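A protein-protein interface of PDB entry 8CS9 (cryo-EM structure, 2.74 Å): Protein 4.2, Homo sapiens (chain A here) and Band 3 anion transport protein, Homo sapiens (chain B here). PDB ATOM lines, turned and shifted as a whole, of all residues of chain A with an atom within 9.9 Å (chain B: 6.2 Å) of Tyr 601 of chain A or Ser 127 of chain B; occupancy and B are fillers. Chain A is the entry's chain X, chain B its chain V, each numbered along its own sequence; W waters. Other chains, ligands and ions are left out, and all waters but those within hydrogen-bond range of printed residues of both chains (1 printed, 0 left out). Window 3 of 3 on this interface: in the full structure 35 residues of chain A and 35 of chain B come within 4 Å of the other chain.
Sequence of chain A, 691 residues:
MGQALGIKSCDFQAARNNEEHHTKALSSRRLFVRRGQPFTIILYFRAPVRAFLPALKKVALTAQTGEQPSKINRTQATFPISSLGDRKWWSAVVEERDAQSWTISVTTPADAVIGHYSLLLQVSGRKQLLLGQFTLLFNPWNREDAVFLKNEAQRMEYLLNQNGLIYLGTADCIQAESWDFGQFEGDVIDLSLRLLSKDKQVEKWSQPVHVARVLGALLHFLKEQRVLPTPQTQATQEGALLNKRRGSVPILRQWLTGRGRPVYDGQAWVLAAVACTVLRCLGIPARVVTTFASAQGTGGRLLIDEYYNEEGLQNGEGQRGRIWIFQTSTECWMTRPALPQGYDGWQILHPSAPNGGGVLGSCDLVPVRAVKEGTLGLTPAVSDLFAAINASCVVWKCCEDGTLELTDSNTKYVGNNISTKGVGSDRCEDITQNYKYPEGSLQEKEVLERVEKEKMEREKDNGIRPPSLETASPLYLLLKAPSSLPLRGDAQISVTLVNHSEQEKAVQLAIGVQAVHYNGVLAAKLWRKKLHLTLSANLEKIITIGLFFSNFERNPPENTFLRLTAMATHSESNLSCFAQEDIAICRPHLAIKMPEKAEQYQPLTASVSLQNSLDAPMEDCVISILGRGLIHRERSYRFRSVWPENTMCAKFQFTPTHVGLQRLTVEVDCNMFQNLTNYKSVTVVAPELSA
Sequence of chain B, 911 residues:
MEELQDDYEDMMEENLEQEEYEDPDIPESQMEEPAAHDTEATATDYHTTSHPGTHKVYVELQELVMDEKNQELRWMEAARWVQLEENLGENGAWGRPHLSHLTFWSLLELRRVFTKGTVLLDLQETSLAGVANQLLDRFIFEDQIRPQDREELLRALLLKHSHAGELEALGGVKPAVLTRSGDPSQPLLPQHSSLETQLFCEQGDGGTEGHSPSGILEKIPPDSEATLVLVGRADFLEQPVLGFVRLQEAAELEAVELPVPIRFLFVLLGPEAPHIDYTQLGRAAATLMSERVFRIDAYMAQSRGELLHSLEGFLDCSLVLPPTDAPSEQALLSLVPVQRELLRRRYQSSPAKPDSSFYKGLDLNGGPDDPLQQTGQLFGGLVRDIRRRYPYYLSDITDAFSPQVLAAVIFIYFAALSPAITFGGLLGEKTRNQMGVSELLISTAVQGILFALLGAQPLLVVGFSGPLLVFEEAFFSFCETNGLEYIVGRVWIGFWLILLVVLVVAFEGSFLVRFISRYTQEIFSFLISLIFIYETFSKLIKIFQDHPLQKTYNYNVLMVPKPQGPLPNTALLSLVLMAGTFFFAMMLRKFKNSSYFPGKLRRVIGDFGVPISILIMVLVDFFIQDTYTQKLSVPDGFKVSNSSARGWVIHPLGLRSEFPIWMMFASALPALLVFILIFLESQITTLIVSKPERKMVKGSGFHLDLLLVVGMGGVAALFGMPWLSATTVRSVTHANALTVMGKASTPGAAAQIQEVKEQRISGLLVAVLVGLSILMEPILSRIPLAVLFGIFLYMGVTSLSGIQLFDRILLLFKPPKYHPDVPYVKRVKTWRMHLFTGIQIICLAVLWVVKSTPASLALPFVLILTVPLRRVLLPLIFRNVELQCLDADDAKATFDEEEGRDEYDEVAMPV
Val 684 of chain A touches none of the printed residues of chain B. Printed residues of chain A within 4 Å of Glu 125 of chain B: Thr 657 (3.3 Å) and His 658 (3.1 Å). No residue of chain A comes within 4 Å of Thr 126 of chain B. Of chain A, only Tyr 601 comes within 4 Å of Ser 127 of chain B. No residue of chain A comes within 4 Å of Ala 129 of chain B. Of the printed residues of chain A, Asn 133 of chain B touches Tyr 601 (3.9 Å) and Thr 655 (3.6 Å).
Water W1 bridges O of Thr 655 of chain A (2.9 Å) and O of Asn 133 of chain B (3.4 Å).
The side-chain hydroxyl of Thr 657 of chain A sits close to the side-chain carboxylate of Glu 125 of chain B, at 3.4 Å. The side-chain hydroxyl (OG) of Ser 127 of chain B sits at hydrogen-bond distance from the side-chain hydroxyl (OH) of Tyr 601 of chain A (3.0 Å). A ring nitrogen (NE2) of His 658 of chain A lies close to the side-chain carboxylate (OE1) of Glu 125 of chain B (3.3 Å).
The backbone carbonyl oxygen of Ala 129 of chain B lies within hydrogen-bond range of the side-chain amide nitrogen of Asn 133 of chain B, at 2.8 Å. The side-chain hydroxyl (OG) of Ser 127 of chain B sits close to the backbone NH (N) of Ala 129 of chain B, 3.4 Å away. NE2 of Gln 600 of chain A sits at hydrogen-bond distance from O of Thr 657 of chain A. The side-chain hydroxyl (OG1) of Thr 657 of chain A sits at hydrogen-bond distance from a ring nitrogen (ND1) of His 658 of chain A. O of Gly 629 of chain A sits at hydrogen-bond distance from ND1 of His 658 of chain A (3.4 Å). The side-chain hydroxyl (OG) of Ser 127 of chain B sits at hydrogen-bond distance from the backbone NH (N) of Gly 130 of chain B.
Tyr 601 of chain A touches Gly 130 of chain B (CE1 to N, 3.6 Å). ND2 of Asn 133 of chain B touches CB of Tyr 601 of chain A, at 3.9 Å. Asn 133 of chain B touches Thr 655 of chain A (CG to CG2, 3.6 Å). Gly 130 of chain B touches Thr 657 of chain A (CA to CG2, 3.6 Å).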
ATOM      1  N   SER A  28      35.911 -36.301 -16.038  1.00  0.00           N
ATOM      2  CA  SER A  28      35.446 -36.133 -17.406  1.00  0.00           C
ATOM      3  C   SER A  28      36.606 -36.007 -18.383  1.00  0.00           C
ATOM      4  O   SER A  28      36.385 -35.724 -19.563  1.00  0.00           O
ATOM      5  CB  SER A  28      34.532 -34.911 -17.517  1.00  0.00           C
ATOM      6  OG  SER A  28      33.722 -34.773 -16.365  1.00  0.00           O
ATOM      7  N   ALA A 598      15.142 -28.229  -5.611  1.00  0.00           N
ATOM      8  CA  ALA A 598      15.797 -26.956  -5.867  1.00  0.00           C
ATOM      9  C   ALA A 598      16.266 -26.917  -7.312  1.00  0.00           C
ATOM     10  O   ALA A 598      16.664 -27.936  -7.878  1.00  0.00           O
ATOM     11  CB  ALA A 598      16.983 -26.727  -4.923  1.00  0.00           C
ATOM     12  N   GLU A 599      16.210 -25.732  -7.908  1.00  0.00           N
ATOM     13  CA  GLU A 599      16.701 -25.549  -9.264  1.00  0.00           C
ATOM     14  C   GLU A 599      18.203 -25.301  -9.254  1.00  0.00           C
ATOM     15  O   GLU A 599      18.733 -24.601  -8.389  1.00  0.00           O
ATOM     16  CB  GLU A 599      15.994 -24.388  -9.961  1.00  0.00           C
ATOM     17  CG  GLU A 599      16.089 -24.451 -11.476  1.00  0.00           C
ATOM     18  CD  GLU A 599      15.498 -23.235 -12.159  1.00  0.00           C
ATOM     19  OE1 GLU A 599      14.457 -22.731 -11.689  1.00  0.00           O
ATOM     20  OE2 GLU A 599      16.073 -22.787 -13.173  1.00  0.00           O
ATOM     21  N   GLN A 600      18.886 -25.896 -10.226  1.00  0.00           N
ATOM     22  CA  GLN A 600      20.312 -25.682 -10.396  1.00  0.00           C
ATOM     23  C   GLN A 600      20.573 -24.242 -10.817  1.00  0.00           C
ATOM     24  O   GLN A 600      19.794 -23.651 -11.569  1.00  0.00           O
ATOM     25  CB  GLN A 600      20.873 -26.654 -11.435  1.00  0.00           C
ATOM     26  CG  GLN A 600      22.384 -26.715 -11.500  1.00  0.00           C
ATOM     27  CD  GLN A 600      22.882 -27.428 -12.734  1.00  0.00           C
ATOM     28  OE1 GLN A 600      22.158 -27.567 -13.715  1.00  0.00           O
ATOM     29  NE2 GLN A 600      24.125 -27.879 -12.695  1.00  0.00           N
ATOM     30  N   TYR A 601      21.665 -23.676 -10.304  1.00  0.00           N
ATOM     31  CA  TYR A 601      22.134 -22.312 -10.563  1.00  0.00           C
ATOM     32  C   TYR A 601      21.166 -21.251 -10.059  1.00  0.00           C
ATOM     33  O   TYR A 601      21.212 -20.113 -10.539  1.00  0.00           O
ATOM     34  CB  TYR A 601      22.417 -22.069 -12.048  1.00  0.00           C
ATOM     35  CG  TYR A 601      23.358 -23.080 -12.656  1.00  0.00           C
ATOM     36  CD1 TYR A 601      24.484 -23.505 -11.972  1.00  0.00           C
ATOM     37  CD2 TYR A 601      23.119 -23.609 -13.913  1.00  0.00           C
ATOM     38  CE1 TYR A 601      25.345 -24.422 -12.522  1.00  0.00           C
ATOM     39  CE2 TYR A 601      23.974 -24.527 -14.472  1.00  0.00           C
ATOM     40  CZ  TYR A 601      25.086 -24.931 -13.775  1.00  0.00           C
ATOM     41  OH  TYR A 601      25.940 -25.850 -14.334  1.00  0.00           O
ATOM     42  N   GLN A 602      20.302 -21.578  -9.100  1.00  0.00           N
ATOM     43  CA  GLN A 602      19.393 -20.628  -8.486  1.00  0.00           C
ATOM     44  C   GLN A 602      19.616 -20.601  -6.979  1.00  0.00           C
ATOM     45  O   GLN A 602      19.904 -21.642  -6.385  1.00  0.00           O
ATOM     46  CB  GLN A 602      17.932 -20.990  -8.785  1.00  0.00           C
ATOM     47  CG  GLN A 602      17.215 -20.004  -9.687  1.00  0.00           C
ATOM     48  CD  GLN A 602      17.856 -19.877 -11.051  1.00  0.00           C
ATOM     49  OE1 GLN A 602      17.744 -20.773 -11.886  1.00  0.00           O
ATOM     50  NE2 GLN A 602      18.528 -18.759 -11.287  1.00  0.00           N
ATOM     51  N   PRO A 603      19.511 -19.436  -6.338  1.00  0.00           N
ATOM     52  CA  PRO A 603      19.789 -19.366  -4.898  1.00  0.00           C
ATOM     53  C   PRO A 603      18.770 -20.148  -4.083  1.00  0.00           C
ATOM     54  O   PRO A 603      17.577 -20.167  -4.392  1.00  0.00           O
ATOM     55  CB  PRO A 603      19.724 -17.865  -4.594  1.00  0.00           C
ATOM     56  CG  PRO A 603      18.906 -17.287  -5.684  1.00  0.00           C
ATOM     57  CD  PRO A 603      19.157 -18.123  -6.900  1.00  0.00           C
ATOM     58  N   LEU A 604      19.258 -20.793  -3.027  1.00  0.00           N
ATOM     59  CA  LEU A 604      18.452 -21.665  -2.184  1.00  0.00           C
ATOM     60  C   LEU A 604      18.739 -21.345  -0.726  1.00  0.00           C
ATOM     61  O   LEU A 604      19.902 -21.223  -0.334  1.00  0.00           O
ATOM     62  CB  LEU A 604      18.752 -23.139  -2.486  1.00  0.00           C
ATOM     63  CG  LEU A 604      18.200 -24.212  -1.549  1.00  0.00           C
ATOM     64  CD1 LEU A 604      16.756 -24.540  -1.888  1.00  0.00           C
ATOM     65  CD2 LEU A 604      19.061 -25.458  -1.621  1.00  0.00           C
ATOM     66  N   GLY A 629      28.505 -31.022  -3.931  1.00  0.00           N
ATOM     67  CA  GLY A 629      27.538 -30.638  -4.941  1.00  0.00           C
ATOM     68  C   GLY A 629      26.755 -29.384  -4.626  1.00  0.00           C
ATOM     69  O   GLY A 629      26.058 -28.871  -5.513  1.00  0.00           O
ATOM     70  N   LEU A 630      26.827 -28.871  -3.408  1.00  0.00           N
ATOM     71  CA  LEU A 630      26.153 -27.630  -3.046  1.00  0.00           C
ATOM     72  C   LEU A 630      27.114 -26.560  -2.562  1.00  0.00           C
ATOM     73  O   LEU A 630      26.947 -25.389  -2.908  1.00  0.00           O
ATOM     74  CB  LEU A 630      25.095 -27.884  -1.957  1.00  0.00           C
ATOM     75  CG  LEU A 630      24.129 -29.054  -2.114  1.00  0.00           C
ATOM     76  CD1 LEU A 630      23.541 -29.413  -0.766  1.00  0.00           C
ATOM     77  CD2 LEU A 630      23.034 -28.710  -3.095  1.00  0.00           C
ATOM     78  N   PHE A 654      22.688 -20.447  -0.362  1.00  0.00           N
ATOM     79  CA  PHE A 654      23.710 -20.988  -1.240  1.00  0.00           C
ATOM     80  C   PHE A 654      23.048 -21.421  -2.537  1.00  0.00           C
ATOM     81  O   PHE A 654      21.852 -21.718  -2.569  1.00  0.00           O
ATOM     82  CB  PHE A 654      24.463 -22.165  -0.604  1.00  0.00           C
ATOM     83  CG  PHE A 654      23.571 -23.242  -0.058  1.00  0.00           C
ATOM     84  CD1 PHE A 654      23.071 -23.162   1.230  1.00  0.00           C
ATOM     85  CD2 PHE A 654      23.240 -24.341  -0.831  1.00  0.00           C
ATOM     86  CE1 PHE A 654      22.251 -24.150   1.730  1.00  0.00           C
ATOM     87  CE2 PHE A 654      22.423 -25.333  -0.333  1.00  0.00           C
ATOM     88  CZ  PHE A 654      21.927 -25.237   0.948  1.00  0.00           C
ATOM     89  N   THR A 655      23.837 -21.455  -3.605  1.00  0.00           N
ATOM     90  CA  THR A 655      23.324 -21.823  -4.913  1.00  0.00           C
ATOM     91  C   THR A 655      23.771 -23.233  -5.257  1.00  0.00           C
ATOM     92  O   THR A 655      24.983 -23.473  -5.378  1.00  0.00           O
ATOM     93  CB  THR A 655      23.810 -20.842  -5.974  1.00  0.00           C
ATOM     94  OG1 THR A 655      23.151 -19.584  -5.793  1.00  0.00           O
ATOM     95  CG2 THR A 655      23.499 -21.360  -7.352  1.00  0.00           C
ATOM     96  N   PRO A 656      22.857 -24.193  -5.390  1.00  0.00           N
ATOM     97  CA  PRO A 656      23.255 -25.529  -5.851  1.00  0.00           C
ATOM     98  C   PRO A 656      23.717 -25.477  -7.298  1.00  0.00           C
ATOM     99  O   PRO A 656      23.082 -24.846  -8.144  1.00  0.00           O
ATOM    100  CB  PRO A 656      21.976 -26.360  -5.695  1.00  0.00           C
ATOM    101  CG  PRO A 656      21.070 -25.547  -4.840  1.00  0.00           C
ATOM    102  CD  PRO A 656      21.419 -24.124  -5.096  1.00  0.00           C
ATOM    103  N   THR A 657      24.824 -26.156  -7.580  1.00  0.00           N
ATOM    104  CA  THR A 657      25.449 -26.081  -8.888  1.00  0.00           C
ATOM    105  C   THR A 657      25.554 -27.420  -9.601  1.00  0.00           C
ATOM    106  O   THR A 657      25.889 -27.438 -10.790  1.00  0.00           O
ATOM    107  CB  THR A 657      26.852 -25.465  -8.769  1.00  0.00           C
ATOM    108  OG1 THR A 657      27.488 -25.954  -7.584  1.00  0.00           O
ATOM    109  CG2 THR A 657      26.754 -23.954  -8.677  1.00  0.00           C
ATOM    110  N   HIS A 658      25.274 -28.531  -8.925  1.00  0.00           N
ATOM    111  CA  HIS A 658      25.356 -29.859  -9.518  1.00  0.00           C
ATOM    112  C   HIS A 658      23.980 -30.503  -9.488  1.00  0.00           C
ATOM    113  O   HIS A 658      23.309 -30.496  -8.452  1.00  0.00           O
ATOM    114  CB  HIS A 658      26.373 -30.729  -8.782  1.00  0.00           C
ATOM    115  CG  HIS A 658      27.774 -30.218  -8.871  1.00  0.00           C
ATOM    116  ND1 HIS A 658      28.288 -29.306  -7.976  1.00  0.00           N
ATOM    117  CD2 HIS A 658      28.767 -30.486  -9.750  1.00  0.00           C
ATOM    118  CE1 HIS A 658      29.540 -29.037  -8.298  1.00  0.00           C
ATOM    119  NE2 HIS A 658      29.855 -29.740  -9.370  1.00  0.00           N
ATOM    120  N   VAL A 659      23.569 -31.061 -10.626  1.00  0.00           N
ATOM    121  CA  VAL A 659      22.274 -31.716 -10.722  1.00  0.00           C
ATOM    122  C   VAL A 659      22.349 -33.102 -10.092  1.00  0.00           C
ATOM    123  O   VAL A 659      23.318 -33.849 -10.284  1.00  0.00           O
ATOM    124  CB  VAL A 659      21.833 -31.781 -12.196  1.00  0.00           C
ATOM    125  CG1 VAL A 659      21.053 -33.057 -12.496  1.00  0.00           C
ATOM    126  CG2 VAL A 659      21.015 -30.560 -12.552  1.00  0.00           C
ATOM    127  N   GLY A 660      21.328 -33.444  -9.311  1.00  0.00           N
ATOM    128  CA  GLY A 660      21.199 -34.759  -8.727  1.00  0.00           C
ATOM    129  C   GLY A 660      20.647 -34.685  -7.326  1.00  0.00           C
ATOM    130  O   GLY A 660      20.177 -33.640  -6.865  1.00  0.00           O
ATOM    131  N   VAL A 684      18.412 -31.546  -6.608  1.00  0.00           N
ATOM    132  CA  VAL A 684      18.692 -30.408  -7.475  1.00  0.00           C
ATOM    133  C   VAL A 684      18.356 -30.804  -8.904  1.00  0.00           C
ATOM    134  O   VAL A 684      18.888 -31.792  -9.424  1.00  0.00           O
ATOM    135  CB  VAL A 684      20.157 -29.955  -7.351  1.00  0.00           C
ATOM    136  CG1 VAL A 684      20.393 -28.704  -8.175  1.00  0.00           C
ATOM    137  CG2 VAL A 684      20.509 -29.713  -5.898  1.00  0.00           C
ATOM    138  N   VAL A 685      17.479 -30.035  -9.540  1.00  0.00           N
ATOM    139  CA  VAL A 685      16.972 -30.367 -10.864  1.00  0.00           C
ATOM    140  C   VAL A 685      17.559 -29.406 -11.886  1.00  0.00           C
ATOM    141  O   VAL A 685      17.958 -28.281 -11.564  1.00  0.00           O
ATOM    142  CB  VAL A 685      15.428 -30.349 -10.901  1.00  0.00           C
ATOM    143  CG1 VAL A 685      14.871 -31.099  -9.708  1.00  0.00           C
ATOM    144  CG2 VAL A 685      14.901 -28.923 -10.921  1.00  0.00           C
ATOM    145  N   ALA A 686      17.629 -29.872 -13.129  1.00  0.00           N
ATOM    146  CA  ALA A 686      18.151 -29.058 -14.210  1.00  0.00           C
ATOM    147  C   ALA A 686      17.182 -27.920 -14.530  1.00  0.00           C
ATOM    148  O   ALA A 686      15.973 -28.052 -14.333  1.00  0.00           O
ATOM    149  CB  ALA A 686      18.386 -29.918 -15.450  1.00  0.00           C
ATOM    150  N   PRO A 687      17.690 -26.784 -15.011  1.00  0.00           N
ATOM    151  CA  PRO A 687      16.795 -25.672 -15.349  1.00  0.00           C
ATOM    152  C   PRO A 687      15.907 -26.013 -16.534  1.00  0.00           C
ATOM    153  O   PRO A 687      16.255 -26.833 -17.387  1.00  0.00           O
ATOM    154  CB  PRO A 687      17.753 -24.519 -15.677  1.00  0.00           C
ATOM    155  CG  PRO A 687      19.113 -24.977 -15.265  1.00  0.00           C
ATOM    156  CD  PRO A 687      19.101 -26.461 -15.277  1.00  0.00           C
ATOM    157  N   GLU A 688      14.737 -25.378 -16.570  1.00  0.00           N
ATOM    158  CA  GLU A 688      13.783 -25.625 -17.641  1.00  0.00           C
ATOM    159  C   GLU A 688      14.340 -25.143 -18.975  1.00  0.00           C
ATOM    160  O   GLU A 688      14.943 -24.071 -19.066  1.00  0.00           O
ATOM    161  CB  GLU A 688      12.457 -24.927 -17.338  1.00  0.00           C
ATOM    162  CG  GLU A 688      11.257 -25.541 -18.041  1.00  0.00           C
ATOM    163  CD  GLU A 688      10.789 -26.822 -17.380  1.00  0.00           C
ATOM    164  OE1 GLU A 688      10.117 -26.741 -16.330  1.00  0.00           O
ATOM    165  OE2 GLU A 688      11.093 -27.912 -17.909  1.00  0.00           O
ATOM    166  N   GLU B 125      33.940 -27.908 -10.561  1.00  0.00           N
ATOM    167  CA  GLU B 125      32.977 -27.230 -11.409  1.00  0.00           C
ATOM    168  C   GLU B 125      33.373 -27.396 -12.866  1.00  0.00           C
ATOM    169  O   GLU B 125      34.557 -27.489 -13.198  1.00  0.00           O
ATOM    170  CB  GLU B 125      32.875 -25.749 -11.046  1.00  0.00           C
ATOM    171  CG  GLU B 125      31.456 -25.243 -10.968  1.00  0.00           C
ATOM    172  CD  GLU B 125      30.680 -25.855  -9.824  1.00  0.00           C
ATOM    173  OE1 GLU B 125      29.653 -26.509 -10.090  1.00  0.00           O
ATOM    174  OE2 GLU B 125      31.096 -25.684  -8.660  1.00  0.00           O
ATOM    175  N   THR B 126      32.361 -27.429 -13.738  1.00  0.00           N
ATOM    176  CA  THR B 126      32.593 -27.675 -15.155  1.00  0.00           C
ATOM    177  C   THR B 126      31.810 -26.732 -16.060  1.00  0.00           C
ATOM    178  O   THR B 126      31.742 -26.978 -17.270  1.00  0.00           O
ATOM    179  CB  THR B 126      32.248 -29.126 -15.511  1.00  0.00           C
ATOM    180  OG1 THR B 126      31.380 -29.671 -14.511  1.00  0.00           O
ATOM    181  CG2 THR B 126      33.511 -29.965 -15.586  1.00  0.00           C
ATOM    182  N   SER B 127      31.211 -25.676 -15.521  1.00  0.00           N
ATOM    183  CA  SER B 127      30.499 -24.689 -16.317  1.00  0.00           C
ATOM    184  C   SER B 127      30.766 -23.307 -15.742  1.00  0.00           C
ATOM    185  O   SER B 127      31.083 -23.158 -14.560  1.00  0.00           O
ATOM    186  CB  SER B 127      28.992 -24.968 -16.353  1.00  0.00           C
ATOM    187  OG  SER B 127      28.323 -24.306 -15.297  1.00  0.00           O
ATOM    188  N   LEU B 128      30.639 -22.289 -16.594  1.00  0.00           N
ATOM    189  CA  LEU B 128      30.875 -20.923 -16.140  1.00  0.00           C
ATOM    190  C   LEU B 128      29.840 -20.493 -15.111  1.00  0.00           C
ATOM    191  O   LEU B 128      30.163 -19.754 -14.176  1.00  0.00           O
ATOM    192  CB  LEU B 128      30.879 -19.956 -17.323  1.00  0.00           C
ATOM    193  CG  LEU B 128      31.354 -18.546 -16.961  1.00  0.00           C
ATOM    194  CD1 LEU B 128      32.724 -18.597 -16.304  1.00  0.00           C
ATOM    195  CD2 LEU B 128      31.369 -17.631 -18.168  1.00  0.00           C
ATOM    196  N   ALA B 129      28.589 -20.934 -15.271  1.00  0.00           N
ATOM    197  CA  ALA B 129      27.548 -20.569 -14.314  1.00  0.00           C
ATOM    198  C   ALA B 129      27.862 -21.104 -12.925  1.00  0.00           C
ATOM    199  O   ALA B 129      27.720 -20.385 -11.929  1.00  0.00           O
ATOM    200  CB  ALA B 129      26.193 -21.078 -14.798  1.00  0.00           C
ATOM    201  N   GLY B 130      28.314 -22.357 -12.839  1.00  0.00           N
ATOM    202  CA  GLY B 130      28.656 -22.922 -11.544  1.00  0.00           C
ATOM    203  C   GLY B 130      29.856 -22.246 -10.904  1.00  0.00           C
ATOM    204  O   GLY B 130      29.851 -21.951  -9.704  1.00  0.00           O
ATOM    205  N   VAL B 131      30.904 -22.005 -11.698  1.00  0.00           N
ATOM    206  CA  VAL B 131      32.087 -21.309 -11.198  1.00  0.00           C
ATOM    207  C   VAL B 131      31.713 -19.927 -10.689  1.00  0.00           C
ATOM    208  O   VAL B 131      32.135 -19.517  -9.603  1.00  0.00           O
ATOM    209  CB  VAL B 131      33.168 -21.230 -12.293  1.00  0.00           C
ATOM    210  CG1 VAL B 131      34.354 -20.420 -11.811  1.00  0.00           C
ATOM    211  CG2 VAL B 131      33.619 -22.614 -12.701  1.00  0.00           C
ATOM    212  N   ALA B 132      30.902 -19.197 -11.458  1.00  0.00           N
ATOM    213  CA  ALA B 132      30.484 -17.859 -11.061  1.00  0.00           C
ATOM    214  C   ALA B 132      29.648 -17.888  -9.788  1.00  0.00           C
ATOM    215  O   ALA B 132      29.840 -17.052  -8.900  1.00  0.00           O
ATOM    216  CB  ALA B 132      29.710 -17.197 -12.198  1.00  0.00           C
ATOM    217  N   ASN B 133      28.725 -18.844  -9.677  1.00  0.00           N
ATOM    218  CA  ASN B 133      27.881 -18.915  -8.489  1.00  0.00           C
ATOM    219  C   ASN B 133      28.693 -19.235  -7.240  1.00  0.00           C
ATOM    220  O   ASN B 133      28.526 -18.584  -6.201  1.00  0.00           O
ATOM    221  CB  ASN B 133      26.774 -19.944  -8.699  1.00  0.00           C
ATOM    222  CG  ASN B 133      25.590 -19.374  -9.441  1.00  0.00           C
ATOM    223  OD1 ASN B 133      24.909 -18.482  -8.945  1.00  0.00           O
ATOM    224  ND2 ASN B 133      25.333 -19.889 -10.633  1.00  0.00           N
ATOM    225  N   LEU B 154      26.499 -11.612 -10.892  1.00  0.00           N
ATOM    226  CA  LEU B 154      26.166 -12.833 -11.618  1.00  0.00           C
ATOM    227  C   LEU B 154      25.673 -12.520 -13.022  1.00  0.00           C
ATOM    228  O   LEU B 154      26.033 -13.214 -13.979  1.00  0.00           O
ATOM    229  CB  LEU B 154      25.113 -13.630 -10.845  1.00  0.00           C
ATOM    230  CG  LEU B 154      24.842 -15.075 -11.271  1.00  0.00           C
ATOM    231  CD1 LEU B 154      26.105 -15.914 -11.220  1.00  0.00           C
ATOM    232  CD2 LEU B 154      23.755 -15.682 -10.405  1.00  0.00           C
ATOM    233  N   ALA B 251      38.400 -27.902 -17.851  1.00  0.00           N
ATOM    234  CA  ALA B 251      37.045 -27.952 -18.369  1.00  0.00           C
ATOM    235  C   ALA B 251      36.929 -27.102 -19.624  1.00  0.00           C
ATOM    236  O   ALA B 251      37.552 -26.044 -19.738  1.00  0.00           O
ATOM    237  CB  ALA B 251      36.032 -27.476 -17.324  1.00  0.00           C
ATOM    238  N   LEU B 253      34.515 -24.945 -20.988  1.00  0.00           N
ATOM    239  CA  LEU B 253      33.302 -24.215 -20.655  1.00  0.00           C
ATOM    240  C   LEU B 253      32.545 -23.851 -21.926  1.00  0.00           C
ATOM    241  O   LEU B 253      33.139 -23.400 -22.908  1.00  0.00           O
ATOM    242  CB  LEU B 253      33.644 -22.962 -19.850  1.00  0.00           C
ATOM    243  CG  LEU B 253      34.509 -23.182 -18.605  1.00  0.00           C
ATOM    244  CD1 LEU B 253      34.707 -21.887 -17.833  1.00  0.00           C
ATOM    245  CD2 LEU B 253      33.914 -24.248 -17.706  1.00  0.00           C
ATOM    246  N   GLU B 254      31.231 -24.076 -21.917  1.00  0.00           N
ATOM    247  CA  GLU B 254      30.431 -23.771 -23.099  1.00  0.00           C
ATOM    248  C   GLU B 254      30.220 -22.271 -23.252  1.00  0.00           C
ATOM    249  O   GLU B 254      30.075 -21.773 -24.375  1.00  0.00           O
ATOM    250  CB  GLU B 254      29.089 -24.498 -23.027  1.00  0.00           C
ATOM    251  CG  GLU B 254      29.170 -25.977 -23.365  1.00  0.00           C
ATOM    252  CD  GLU B 254      29.103 -26.236 -24.858  1.00  0.00           C
ATOM    253  OE1 GLU B 254      28.712 -25.314 -25.604  1.00  0.00           O
ATOM    254  OE2 GLU B 254      29.446 -27.358 -25.284  1.00  0.00           O
HETATM  255  O   HOH W   1      26.974 -21.379  -5.073  1.00  0.00           O
